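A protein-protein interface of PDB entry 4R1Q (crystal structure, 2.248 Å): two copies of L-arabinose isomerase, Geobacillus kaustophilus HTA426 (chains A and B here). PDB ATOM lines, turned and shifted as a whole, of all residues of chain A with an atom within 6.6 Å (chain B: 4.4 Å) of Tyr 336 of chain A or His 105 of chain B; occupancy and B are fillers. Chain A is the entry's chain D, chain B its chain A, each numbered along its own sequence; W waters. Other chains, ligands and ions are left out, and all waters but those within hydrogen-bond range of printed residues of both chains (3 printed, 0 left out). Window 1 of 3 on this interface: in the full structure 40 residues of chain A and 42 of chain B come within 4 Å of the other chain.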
ATOM      1  N   ASP A 333      18.993  -9.824  20.535  1.00  0.00           N
ATOM      2  CA  ASP A 333      18.403 -10.853  19.674  1.00  0.00           C
ATOM      3  C   ASP A 333      18.815 -12.235  20.184  1.00  0.00           C
ATOM      4  O   ASP A 333      20.013 -12.555  20.227  1.00  0.00           O
ATOM      5  CB  ASP A 333      18.895 -10.723  18.232  1.00  0.00           C
ATOM      6  CG  ASP A 333      18.737  -9.320  17.669  1.00  0.00           C
ATOM      7  OD1 ASP A 333      19.487  -8.405  18.090  1.00  0.00           O
ATOM      8  OD2 ASP A 333      17.887  -9.143  16.770  1.00  0.00           O
ATOM      9  N   TYR A 334      17.853 -13.066  20.557  1.00  0.00           N
ATOM     10  CA  TYR A 334      18.231 -14.358  21.130  1.00  0.00           C
ATOM     11  C   TYR A 334      18.108 -15.552  20.197  1.00  0.00           C
ATOM     12  O   TYR A 334      19.060 -16.307  20.061  1.00  0.00           O
ATOM     13  CB  TYR A 334      17.545 -14.626  22.482  1.00  0.00           C
ATOM     14  CG  TYR A 334      18.558 -14.827  23.599  1.00  0.00           C
ATOM     15  CD1 TYR A 334      18.945 -13.757  24.411  1.00  0.00           C
ATOM     16  CD2 TYR A 334      19.161 -16.072  23.815  1.00  0.00           C
ATOM     17  CE1 TYR A 334      19.880 -13.920  25.427  1.00  0.00           C
ATOM     18  CE2 TYR A 334      20.102 -16.250  24.830  1.00  0.00           C
ATOM     19  CZ  TYR A 334      20.452 -15.162  25.635  1.00  0.00           C
ATOM     20  OH  TYR A 334      21.370 -15.298  26.643  1.00  0.00           O
ATOM     21  N   THR A 335      16.959 -15.714  19.541  1.00  0.00           N
ATOM     22  CA  THR A 335      16.748 -16.856  18.645  1.00  0.00           C
ATOM     23  C   THR A 335      15.658 -16.534  17.612  1.00  0.00           C
ATOM     24  O   THR A 335      14.861 -15.609  17.820  1.00  0.00           O
ATOM     25  CB  THR A 335      16.414 -18.154  19.450  1.00  0.00           C
ATOM     26  OG1 THR A 335      16.476 -19.295  18.587  1.00  0.00           O
ATOM     27  CG2 THR A 335      15.031 -18.068  20.098  1.00  0.00           C
ATOM     28  N   TYR A 336      15.636 -17.279  16.505  1.00  0.00           N
ATOM     29  CA  TYR A 336      14.762 -16.971  15.370  1.00  0.00           C
ATOM     30  C   TYR A 336      13.624 -17.972  15.180  1.00  0.00           C
ATOM     31  O   TYR A 336      13.765 -19.165  15.461  1.00  0.00           O
ATOM     32  CB  TYR A 336      15.546 -16.943  14.049  1.00  0.00           C
ATOM     33  CG  TYR A 336      16.506 -15.784  13.828  1.00  0.00           C
ATOM     34  CD1 TYR A 336      16.409 -14.594  14.547  1.00  0.00           C
ATOM     35  CD2 TYR A 336      17.508 -15.881  12.873  1.00  0.00           C
ATOM     36  CE1 TYR A 336      17.305 -13.534  14.318  1.00  0.00           C
ATOM     37  CE2 TYR A 336      18.404 -14.831  12.644  1.00  0.00           C
ATOM     38  CZ  TYR A 336      18.298 -13.664  13.365  1.00  0.00           C
ATOM     39  OH  TYR A 336      19.196 -12.644  13.122  1.00  0.00           O
ATOM     40  N   HIS A 337      12.506 -17.463  14.665  1.00  0.00           N
ATOM     41  CA  HIS A 337      11.411 -18.286  14.165  1.00  0.00           C
ATOM     42  C   HIS A 337      11.357 -18.111  12.644  1.00  0.00           C
ATOM     43  O   HIS A 337      10.985 -17.044  12.156  1.00  0.00           O
ATOM     44  CB  HIS A 337      10.098 -17.819  14.810  1.00  0.00           C
ATOM     45  CG  HIS A 337       8.953 -18.771  14.641  1.00  0.00           C
ATOM     46  ND1 HIS A 337       8.983 -20.063  15.117  1.00  0.00           N
ATOM     47  CD2 HIS A 337       7.738 -18.610  14.064  1.00  0.00           C
ATOM     48  CE1 HIS A 337       7.839 -20.662  14.835  1.00  0.00           C
ATOM     49  NE2 HIS A 337       7.066 -19.804  14.195  1.00  0.00           N
ATOM     50  N   PHE A 338      11.745 -19.144  11.901  1.00  0.00           N
ATOM     51  CA  PHE A 338      11.892 -19.036  10.445  1.00  0.00           C
ATOM     52  C   PHE A 338      10.674 -19.564   9.691  1.00  0.00           C
ATOM     53  O   PHE A 338      10.749 -19.830   8.493  1.00  0.00           O
ATOM     54  CB  PHE A 338      13.127 -19.807   9.948  1.00  0.00           C
ATOM     55  CG  PHE A 338      14.405 -19.014   9.959  1.00  0.00           C
ATOM     56  CD1 PHE A 338      15.496 -19.445  10.701  1.00  0.00           C
ATOM     57  CD2 PHE A 338      14.531 -17.849   9.204  1.00  0.00           C
ATOM     58  CE1 PHE A 338      16.686 -18.725  10.700  1.00  0.00           C
ATOM     59  CE2 PHE A 338      15.715 -17.123   9.203  1.00  0.00           C
ATOM     60  CZ  PHE A 338      16.793 -17.562   9.950  1.00  0.00           C
ATOM     61  N   GLU A 339       9.567 -19.743  10.397  1.00  0.00           N
ATOM     62  CA  GLU A 339       8.338 -20.239   9.788  1.00  0.00           C
ATOM     63  C   GLU A 339       7.965 -19.340   8.614  1.00  0.00           C
ATOM     64  O   GLU A 339       7.834 -18.132   8.782  1.00  0.00           O
ATOM     65  CB  GLU A 339       7.209 -20.254  10.824  1.00  0.00           C
ATOM     66  CG  GLU A 339       5.899 -20.869  10.349  1.00  0.00           C
ATOM     67  CD  GLU A 339       4.721 -20.518  11.263  1.00  0.00           C
ATOM     68  OE1 GLU A 339       3.580 -20.916  10.943  1.00  0.00           O
ATOM     69  OE2 GLU A 339       4.930 -19.842  12.298  1.00  0.00           O
ATOM     70  N   LEU A 344      10.120 -14.250  12.632  1.00  0.00           N
ATOM     71  CA  LEU A 344      10.281 -13.293  13.717  1.00  0.00           C
ATOM     72  C   LEU A 344      11.505 -13.571  14.574  1.00  0.00           C
ATOM     73  O   LEU A 344      12.136 -14.635  14.487  1.00  0.00           O
ATOM     74  CB  LEU A 344       9.014 -13.205  14.582  1.00  0.00           C
ATOM     75  CG  LEU A 344       8.476 -14.492  15.228  1.00  0.00           C
ATOM     76  CD1 LEU A 344       9.230 -14.857  16.514  1.00  0.00           C
ATOM     77  CD2 LEU A 344       6.977 -14.376  15.486  1.00  0.00           C
ATOM     78  N   ILE A 345      11.813 -12.587  15.407  1.00  0.00           N
ATOM     79  CA  ILE A 345      12.914 -12.645  16.342  1.00  0.00           C
ATOM     80  C   ILE A 345      12.403 -12.598  17.777  1.00  0.00           C
ATOM     81  O   ILE A 345      11.590 -11.738  18.125  1.00  0.00           O
ATOM     82  CB  ILE A 345      13.859 -11.453  16.128  1.00  0.00           C
ATOM     83  CG1 ILE A 345      14.386 -11.458  14.690  1.00  0.00           C
ATOM     84  CG2 ILE A 345      14.996 -11.459  17.157  1.00  0.00           C
ATOM     85  CD1 ILE A 345      15.360 -10.326  14.415  1.00  0.00           C
ATOM     86  N   LEU A 346      12.881 -13.534  18.595  1.00  0.00           N
ATOM     87  CA  LEU A 346      12.695 -13.489  20.042  1.00  0.00           C
ATOM     88  C   LEU A 346      13.910 -12.793  20.655  1.00  0.00           C
ATOM     89  O   LEU A 346      15.045 -13.230  20.479  1.00  0.00           O
ATOM     90  CB  LEU A 346      12.549 -14.910  20.613  1.00  0.00           C
ATOM     91  CG  LEU A 346      12.197 -15.103  22.098  1.00  0.00           C
ATOM     92  CD1 LEU A 346      11.572 -16.482  22.328  1.00  0.00           C
ATOM     93  CD2 LEU A 346      13.421 -14.939  22.986  1.00  0.00           C
ATOM     94  N   LEU A 433      12.914 -10.395   7.922  1.00  0.00           N
ATOM     95  CA  LEU A 433      13.961 -10.951   8.783  1.00  0.00           C
ATOM     96  C   LEU A 433      15.247 -11.135   7.961  1.00  0.00           C
ATOM     97  O   LEU A 433      16.331 -10.696   8.342  1.00  0.00           O
ATOM     98  CB  LEU A 433      13.494 -12.273   9.403  1.00  0.00           C
ATOM     99  CG  LEU A 433      14.558 -13.143  10.098  1.00  0.00           C
ATOM    100  CD1 LEU A 433      15.204 -12.372  11.203  1.00  0.00           C
ATOM    101  CD2 LEU A 433      13.973 -14.439  10.639  1.00  0.00           C
ATOM    102  N   ALA A 437      18.414  -8.655   8.744  1.00  0.00           N
ATOM    103  CA  ALA A 437      19.592  -9.300   9.342  1.00  0.00           C
ATOM    104  C   ALA A 437      20.835  -9.152   8.454  1.00  0.00           C
ATOM    105  O   ALA A 437      21.941  -8.931   8.954  1.00  0.00           O
ATOM    106  CB  ALA A 437      19.335 -10.756   9.632  1.00  0.00           C
ATOM    107  N   GLU A 438      20.651  -9.254   7.141  1.00  0.00           N
ATOM    108  CA  GLU A 438      21.764  -9.058   6.223  1.00  0.00           C
ATOM    109  C   GLU A 438      22.290  -7.627   6.270  1.00  0.00           C
ATOM    110  O   GLU A 438      23.495  -7.416   6.347  1.00  0.00           O
ATOM    111  CB  GLU A 438      21.396  -9.441   4.787  1.00  0.00           C
ATOM    112  CG  GLU A 438      22.561  -9.189   3.808  1.00  0.00           C
ATOM    113  CD  GLU A 438      22.292  -9.687   2.384  1.00  0.00           C
ATOM    114  OE1 GLU A 438      21.170 -10.185   2.119  1.00  0.00           O
ATOM    115  OE2 GLU A 438      23.222  -9.581   1.544  1.00  0.00           O
ATOM    116  N   ILE A 441      24.187  -6.984   9.560  1.00  0.00           N
ATOM    117  CA  ILE A 441      25.512  -7.598   9.527  1.00  0.00           C
ATOM    118  C   ILE A 441      26.469  -6.830   8.624  1.00  0.00           C
ATOM    119  O   ILE A 441      27.639  -6.639   8.971  1.00  0.00           O
ATOM    120  CB  ILE A 441      25.419  -9.065   9.085  1.00  0.00           C
ATOM    121  CG1 ILE A 441      24.834  -9.919  10.223  1.00  0.00           C
ATOM    122  CG2 ILE A 441      26.766  -9.602   8.681  1.00  0.00           C
ATOM    123  CD1 ILE A 441      24.437 -11.302   9.778  1.00  0.00           C
ATOM    124  N   HIS B 103      29.722 -15.746   4.912  1.00  0.00           N
ATOM    125  CA  HIS B 103      29.138 -15.780   6.226  1.00  0.00           C
ATOM    126  C   HIS B 103      27.682 -16.238   6.084  1.00  0.00           C
ATOM    127  O   HIS B 103      26.838 -15.529   5.531  1.00  0.00           O
ATOM    128  CB  HIS B 103      29.214 -14.403   6.860  1.00  0.00           C
ATOM    129  CG  HIS B 103      28.602 -14.337   8.214  1.00  0.00           C
ATOM    130  ND1 HIS B 103      28.257 -13.146   8.818  1.00  0.00           N
ATOM    131  CD2 HIS B 103      28.273 -15.317   9.090  1.00  0.00           C
ATOM    132  CE1 HIS B 103      27.741 -13.395  10.008  1.00  0.00           C
ATOM    133  NE2 HIS B 103      27.733 -14.703  10.195  1.00  0.00           N
ATOM    134  N   LEU B 104      27.413 -17.450   6.553  1.00  0.00           N
ATOM    135  CA  LEU B 104      26.074 -18.010   6.529  1.00  0.00           C
ATOM    136  C   LEU B 104      25.435 -17.752   7.878  1.00  0.00           C
ATOM    137  O   LEU B 104      25.902 -18.265   8.908  1.00  0.00           O
ATOM    138  CB  LEU B 104      26.121 -19.513   6.247  1.00  0.00           C
ATOM    139  CG  LEU B 104      24.753 -20.181   6.349  1.00  0.00           C
ATOM    140  CD1 LEU B 104      23.805 -19.614   5.287  1.00  0.00           C
ATOM    141  CD2 LEU B 104      24.897 -21.687   6.213  1.00  0.00           C
ATOM    142  N   HIS B 105      24.398 -16.920   7.871  1.00  0.00           N
ATOM    143  CA  HIS B 105      23.623 -16.613   9.058  1.00  0.00           C
ATOM    144  C   HIS B 105      22.396 -17.524   9.068  1.00  0.00           C
ATOM    145  O   HIS B 105      21.401 -17.258   8.409  1.00  0.00           O
ATOM    146  CB  HIS B 105      23.196 -15.145   9.028  1.00  0.00           C
ATOM    147  CG  HIS B 105      22.467 -14.693  10.255  1.00  0.00           C
ATOM    148  ND1 HIS B 105      22.596 -15.320  11.473  1.00  0.00           N
ATOM    149  CD2 HIS B 105      21.599 -13.668  10.452  1.00  0.00           C
ATOM    150  CE1 HIS B 105      21.852 -14.698  12.370  1.00  0.00           C
ATOM    151  NE2 HIS B 105      21.232 -13.694  11.775  1.00  0.00           N
ATOM    152  N   THR B 106      22.478 -18.616   9.808  1.00  0.00           N
ATOM    153  CA  THR B 106      21.432 -19.622   9.766  1.00  0.00           C
ATOM    154  C   THR B 106      21.158 -20.171  11.168  1.00  0.00           C
ATOM    155  O   THR B 106      21.685 -19.666  12.165  1.00  0.00           O
ATOM    156  CB  THR B 106      21.831 -20.763   8.807  1.00  0.00           C
ATOM    157  OG1 THR B 106      20.702 -21.610   8.559  1.00  0.00           O
ATOM    158  CG2 THR B 106      22.987 -21.578   9.385  1.00  0.00           C
ATOM    159  N   GLN B 107      20.337 -21.210  11.245  1.00  0.00           N
ATOM    160  CA  GLN B 107      19.896 -21.748  12.523  1.00  0.00           C
ATOM    161  C   GLN B 107      19.523 -23.191  12.243  1.00  0.00           C
ATOM    162  O   GLN B 107      18.949 -23.473  11.196  1.00  0.00           O
ATOM    163  CB  GLN B 107      18.690 -20.957  13.037  1.00  0.00           C
ATOM    164  CG  GLN B 107      18.212 -21.333  14.430  1.00  0.00           C
ATOM    165  CD  GLN B 107      17.097 -20.423  14.916  1.00  0.00           C
ATOM    166  OE1 GLN B 107      17.342 -19.431  15.608  1.00  0.00           O
ATOM    167  NE2 GLN B 107      15.862 -20.752  14.548  1.00  0.00           N
ATOM    168  N   ARG B 110      14.200 -24.716  12.309  1.00  0.00           N
ATOM    169  CA  ARG B 110      13.440 -23.665  11.659  1.00  0.00           C
ATOM    170  C   ARG B 110      12.642 -22.810  12.659  1.00  0.00           C
ATOM    171  O   ARG B 110      12.696 -21.576  12.615  1.00  0.00           O
ATOM    172  CB  ARG B 110      12.488 -24.265  10.627  1.00  0.00           C
ATOM    173  CG  ARG B 110      12.219 -23.360   9.454  1.00  0.00           C
ATOM    174  CD  ARG B 110      11.088 -23.905   8.599  1.00  0.00           C
ATOM    175  NE  ARG B 110       9.845 -23.880   9.355  1.00  0.00           N
ATOM    176  CZ  ARG B 110       8.657 -24.219   8.869  1.00  0.00           C
ATOM    177  NH1 ARG B 110       7.589 -24.151   9.657  1.00  0.00           N
ATOM    178  NH2 ARG B 110       8.533 -24.619   7.606  1.00  0.00           N
ATOM    179  N   ILE B 112      10.712 -21.843  16.581  1.00  0.00           N
ATOM    180  CA  ILE B 112      10.815 -21.826  18.030  1.00  0.00           C
ATOM    181  C   ILE B 112       9.873 -22.884  18.593  1.00  0.00           C
ATOM    182  O   ILE B 112       8.687 -22.871  18.276  1.00  0.00           O
ATOM    183  CB  ILE B 112      10.432 -20.449  18.608  1.00  0.00           C
ATOM    184  CG1 ILE B 112      11.516 -19.412  18.286  1.00  0.00           C
ATOM    185  CG2 ILE B 112      10.171 -20.543  20.121  1.00  0.00           C
ATOM    186  CD1 ILE B 112      11.127 -17.972  18.620  1.00  0.00           C
ATOM    187  N   SER B 127      22.515 -18.180  17.273  1.00  0.00           N
ATOM    188  CA  SER B 127      23.049 -17.543  16.064  1.00  0.00           C
ATOM    189  C   SER B 127      22.487 -16.136  15.870  1.00  0.00           C
ATOM    190  O   SER B 127      23.157 -15.266  15.312  1.00  0.00           O
ATOM    191  CB  SER B 127      22.688 -18.361  14.830  1.00  0.00           C
ATOM    192  OG  SER B 127      23.417 -19.566  14.786  1.00  0.00           O
ATOM    193  N   ALA B 128      21.250 -15.936  16.317  1.00  0.00           N
ATOM    194  CA  ALA B 128      20.626 -14.617  16.286  1.00  0.00           C
ATOM    195  C   ALA B 128      21.583 -13.561  16.823  1.00  0.00           C
ATOM    196  O   ALA B 128      21.644 -12.487  16.274  1.00  0.00           O
ATOM    197  CB  ALA B 128      19.330 -14.597  17.071  1.00  0.00           C
ATOM    198  N   ASP B 131      26.083 -14.552  15.331  1.00  0.00           N
ATOM    199  CA  ASP B 131      26.357 -14.072  13.969  1.00  0.00           C
ATOM    200  C   ASP B 131      26.426 -12.547  13.824  1.00  0.00           C
ATOM    201  O   ASP B 131      27.010 -12.042  12.863  1.00  0.00           O
ATOM    202  CB  ASP B 131      25.317 -14.616  12.993  1.00  0.00           C
ATOM    203  CG  ASP B 131      25.648 -16.017  12.509  1.00  0.00           C
ATOM    204  OD1 ASP B 131      26.858 -16.293  12.290  1.00  0.00           O
ATOM    205  OD2 ASP B 131      24.696 -16.826  12.342  1.00  0.00           O
ATOM    206  N   ARG B 132      25.828 -11.824  14.766  1.00  0.00           N
ATOM    207  CA  ARG B 132      25.883 -10.362  14.748  1.00  0.00           C
ATOM    208  C   ARG B 132      27.221  -9.839  15.331  1.00  0.00           C
ATOM    209  O   ARG B 132      27.814  -8.898  14.777  1.00  0.00           O
ATOM    210  CB  ARG B 132      24.630  -9.749  15.426  1.00  0.00           C
ATOM    211  CG  ARG B 132      23.328  -9.902  14.573  1.00  0.00           C
ATOM    212  CD  ARG B 132      21.987  -9.780  15.373  1.00  0.00           C
ATOM    213  NE  ARG B 132      21.134  -8.701  14.905  1.00  0.00           N
ATOM    214  CZ  ARG B 132      20.071  -8.805  14.106  1.00  0.00           C
ATOM    215  NH1 ARG B 132      19.625  -9.972  13.650  1.00  0.00           N
ATOM    216  NH2 ARG B 132      19.431  -7.698  13.771  1.00  0.00           N
ATOM    217  N   VAL B 148      24.806 -14.427   3.702  1.00  0.00           N
ATOM    218  CA  VAL B 148      23.594 -15.168   3.344  1.00  0.00           C
ATOM    219  C   VAL B 148      22.773 -15.474   4.607  1.00  0.00           C
ATOM    220  O   VAL B 148      23.277 -16.081   5.563  1.00  0.00           O
ATOM    221  CB  VAL B 148      23.944 -16.485   2.607  1.00  0.00           C
ATOM    222  CG1 VAL B 148      22.694 -17.317   2.349  1.00  0.00           C
ATOM    223  CG2 VAL B 148      24.676 -16.185   1.298  1.00  0.00           C
ATOM    224  N   VAL B 149      21.519 -15.041   4.615  1.00  0.00           N
ATOM    225  CA  VAL B 149      20.660 -15.179   5.784  1.00  0.00           C
ATOM    226  C   VAL B 149      19.489 -16.122   5.490  1.00  0.00           C
ATOM    227  O   VAL B 149      18.891 -16.042   4.421  1.00  0.00           O
ATOM    228  CB  VAL B 149      20.085 -13.814   6.201  1.00  0.00           C
ATOM    229  CG1 VAL B 149      19.163 -13.961   7.428  1.00  0.00           C
ATOM    230  CG2 VAL B 149      21.205 -12.819   6.468  1.00  0.00           C
ATOM    231  N   GLY B 150      19.175 -17.017   6.427  1.00  0.00           N
ATOM    232  CA  GLY B 150      18.030 -17.910   6.284  1.00  0.00           C
ATOM    233  C   GLY B 150      18.271 -19.322   6.808  1.00  0.00           C
ATOM    234  O   GLY B 150      19.395 -19.691   7.120  1.00  0.00           O
HETATM  235  O   HOH W   1      18.063  -6.586  15.781  1.00  0.00           O
HETATM  236  O   HOH W   2      14.575 -20.844  17.493  1.00  0.00           O
HETATM  237  O   HOH W   3      20.699  -6.595  16.761  1.00  0.00           O
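Ala 128 of chain B touches Asp 333 of chain A (O to CB, 3.8 Å).
Tyr 334 of chain A touches Ala 128 of chain B.
Ala 128 of chain B touches Thr 335 of chain A.
Tyr 336 of chain A touches Arg 110 of chain B.
Tyr 336 of chain A touches Ile 112 of chain B.
Phe 338 of chain A touches Gln 107 of chain B (CE1 to CB, 3.8 Å).
CA of Gly 150 of chain B touches CE2 of Phe 338 of chain A (3.8 Å).
His 105 of chain B touches Ala 437 of chain A (CD2 to CB, 3.8 Å).
Val 149 of chain B touches Glu 438 of chain A.
Ile 441 of chain A touches His 103 of chain B (CG2 to ND1, 3.8 Å).
Water W3 lies within hydrogen-bond range of the side-chain carboxylate of Asp 333 of chain A (2.6 Å) and the guanidinium group of Arg 132 of chain B (2.8 Å).
Water W1 bridges NH2 of Arg 132 of chain B (2.7 Å) and OD2 of Asp 333 of chain A (2.7 Å).
Water W2 lies within hydrogen-bond range of OG1 of Thr 335 of chain A, O of Tyr 336 of chain A and NE2 of Gln 107 of chain B.
The side-chain hydroxyl (OG1) of Thr 335 of chain A sits at hydrogen-bond distance from the side-chain amide oxygen (OE1) of Gln 107 of chain B.
The guanidinium group (NH1) of Arg 132 of chain B sits at hydrogen-bond distance from the side-chain hydroxyl (OH) of Tyr 336 of chain A (2.8 Å).
The side-chain carboxylate (OD1) of Asp 333 of chain A lies within salt-bridge range of the guanidinium group (NE) of Arg 132 of chain B, at 3.6 Å.
The backbone carbonyl oxygen (O) of Arg 110 of chain B sits at hydrogen-bond distance from the backbone NH (N) of Phe 338 of chain A (2.7 Å).
NE2 of His 105 of chain B is in hydrogen-bond range of OH of Tyr 336 of chain A.
N of Ile 112 of chain B lies within hydrogen-bond range of ND1 of His 337 of chain A, at 2.9 Å.
The side-chain amide nitrogen of Gln 107 of chain B sits at hydrogen-bond distance from the backbone carbonyl oxygen of Tyr 336 of chain A (2.8 Å).
Among the printed residues, 23 pairs touch across the chains.
Among the printed residues, Asp or Glu carboxylates within 4 Å of a Lys or Arg side-chain nitrogen of the other chain: Asp 333 of chain A with Arg 132 of chain B.
Of chain B, only His 105 (2.7 Å), Gln 107 (2.8 Å), Arg 110 (3.9 Å), Ile 112 (3.6 Å), Ala 128 (3.6 Å) and Arg 132 (2.8 Å) come within 4 Å of Tyr 336 of chain A.
His 105 of chain B touches three residues of chain A.
Printed residues of chain B within 4 Å of Glu 438 of chain A: Val 149 (3.7 Å).
Printed residues of chain B within 4 Å of Tyr 334 of chain A: Ala 128 (3.5 Å).
Printed residues of chain A within 4 Å of His 103 of chain B: Ile 441 (3.8 Å).
Of the printed residues of chain B, Thr 335 of chain A touches Gln 107 (3.1 Å) and Ala 128 (3.6 Å).
Printed residues of chain A within 4 Å of Gly 150 of chain B: Phe 338.
Leu 104 of chain B touches none of the printed residues of chain A.
Leu 344 of chain A touches none of the printed residues of chain B.
No position is printed for both chains.
The backbone carbonyl oxygen (O) of His 103 of chain B lies within hydrogen-bond range of the backbone NH (N) of Val 148 of chain B (2.9 Å).
OD1 of Asp 131 of chain B is in hydrogen-bond range of NE2 of His 103 of chain B (2.8 Å).
The backbone carbonyl oxygen (O) of Thr 335 of chain A lies within hydrogen-bond range of the backbone NH (N) of Leu 346 of chain A (3.0 Å).
O of Val 148 of chain B is in hydrogen-bond range of N of His 105 of chain B, at 2.7 Å.
The side-chain carboxylate (OD2) of Asp 131 of chain B lies within hydrogen-bond range of a ring nitrogen (ND1) of His 105 of chain B, 2.7 Å away.
The side-chain hydroxyl of Thr 106 of chain B lies within hydrogen-bond range of the backbone carbonyl oxygen of Gly 150 of chain B.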
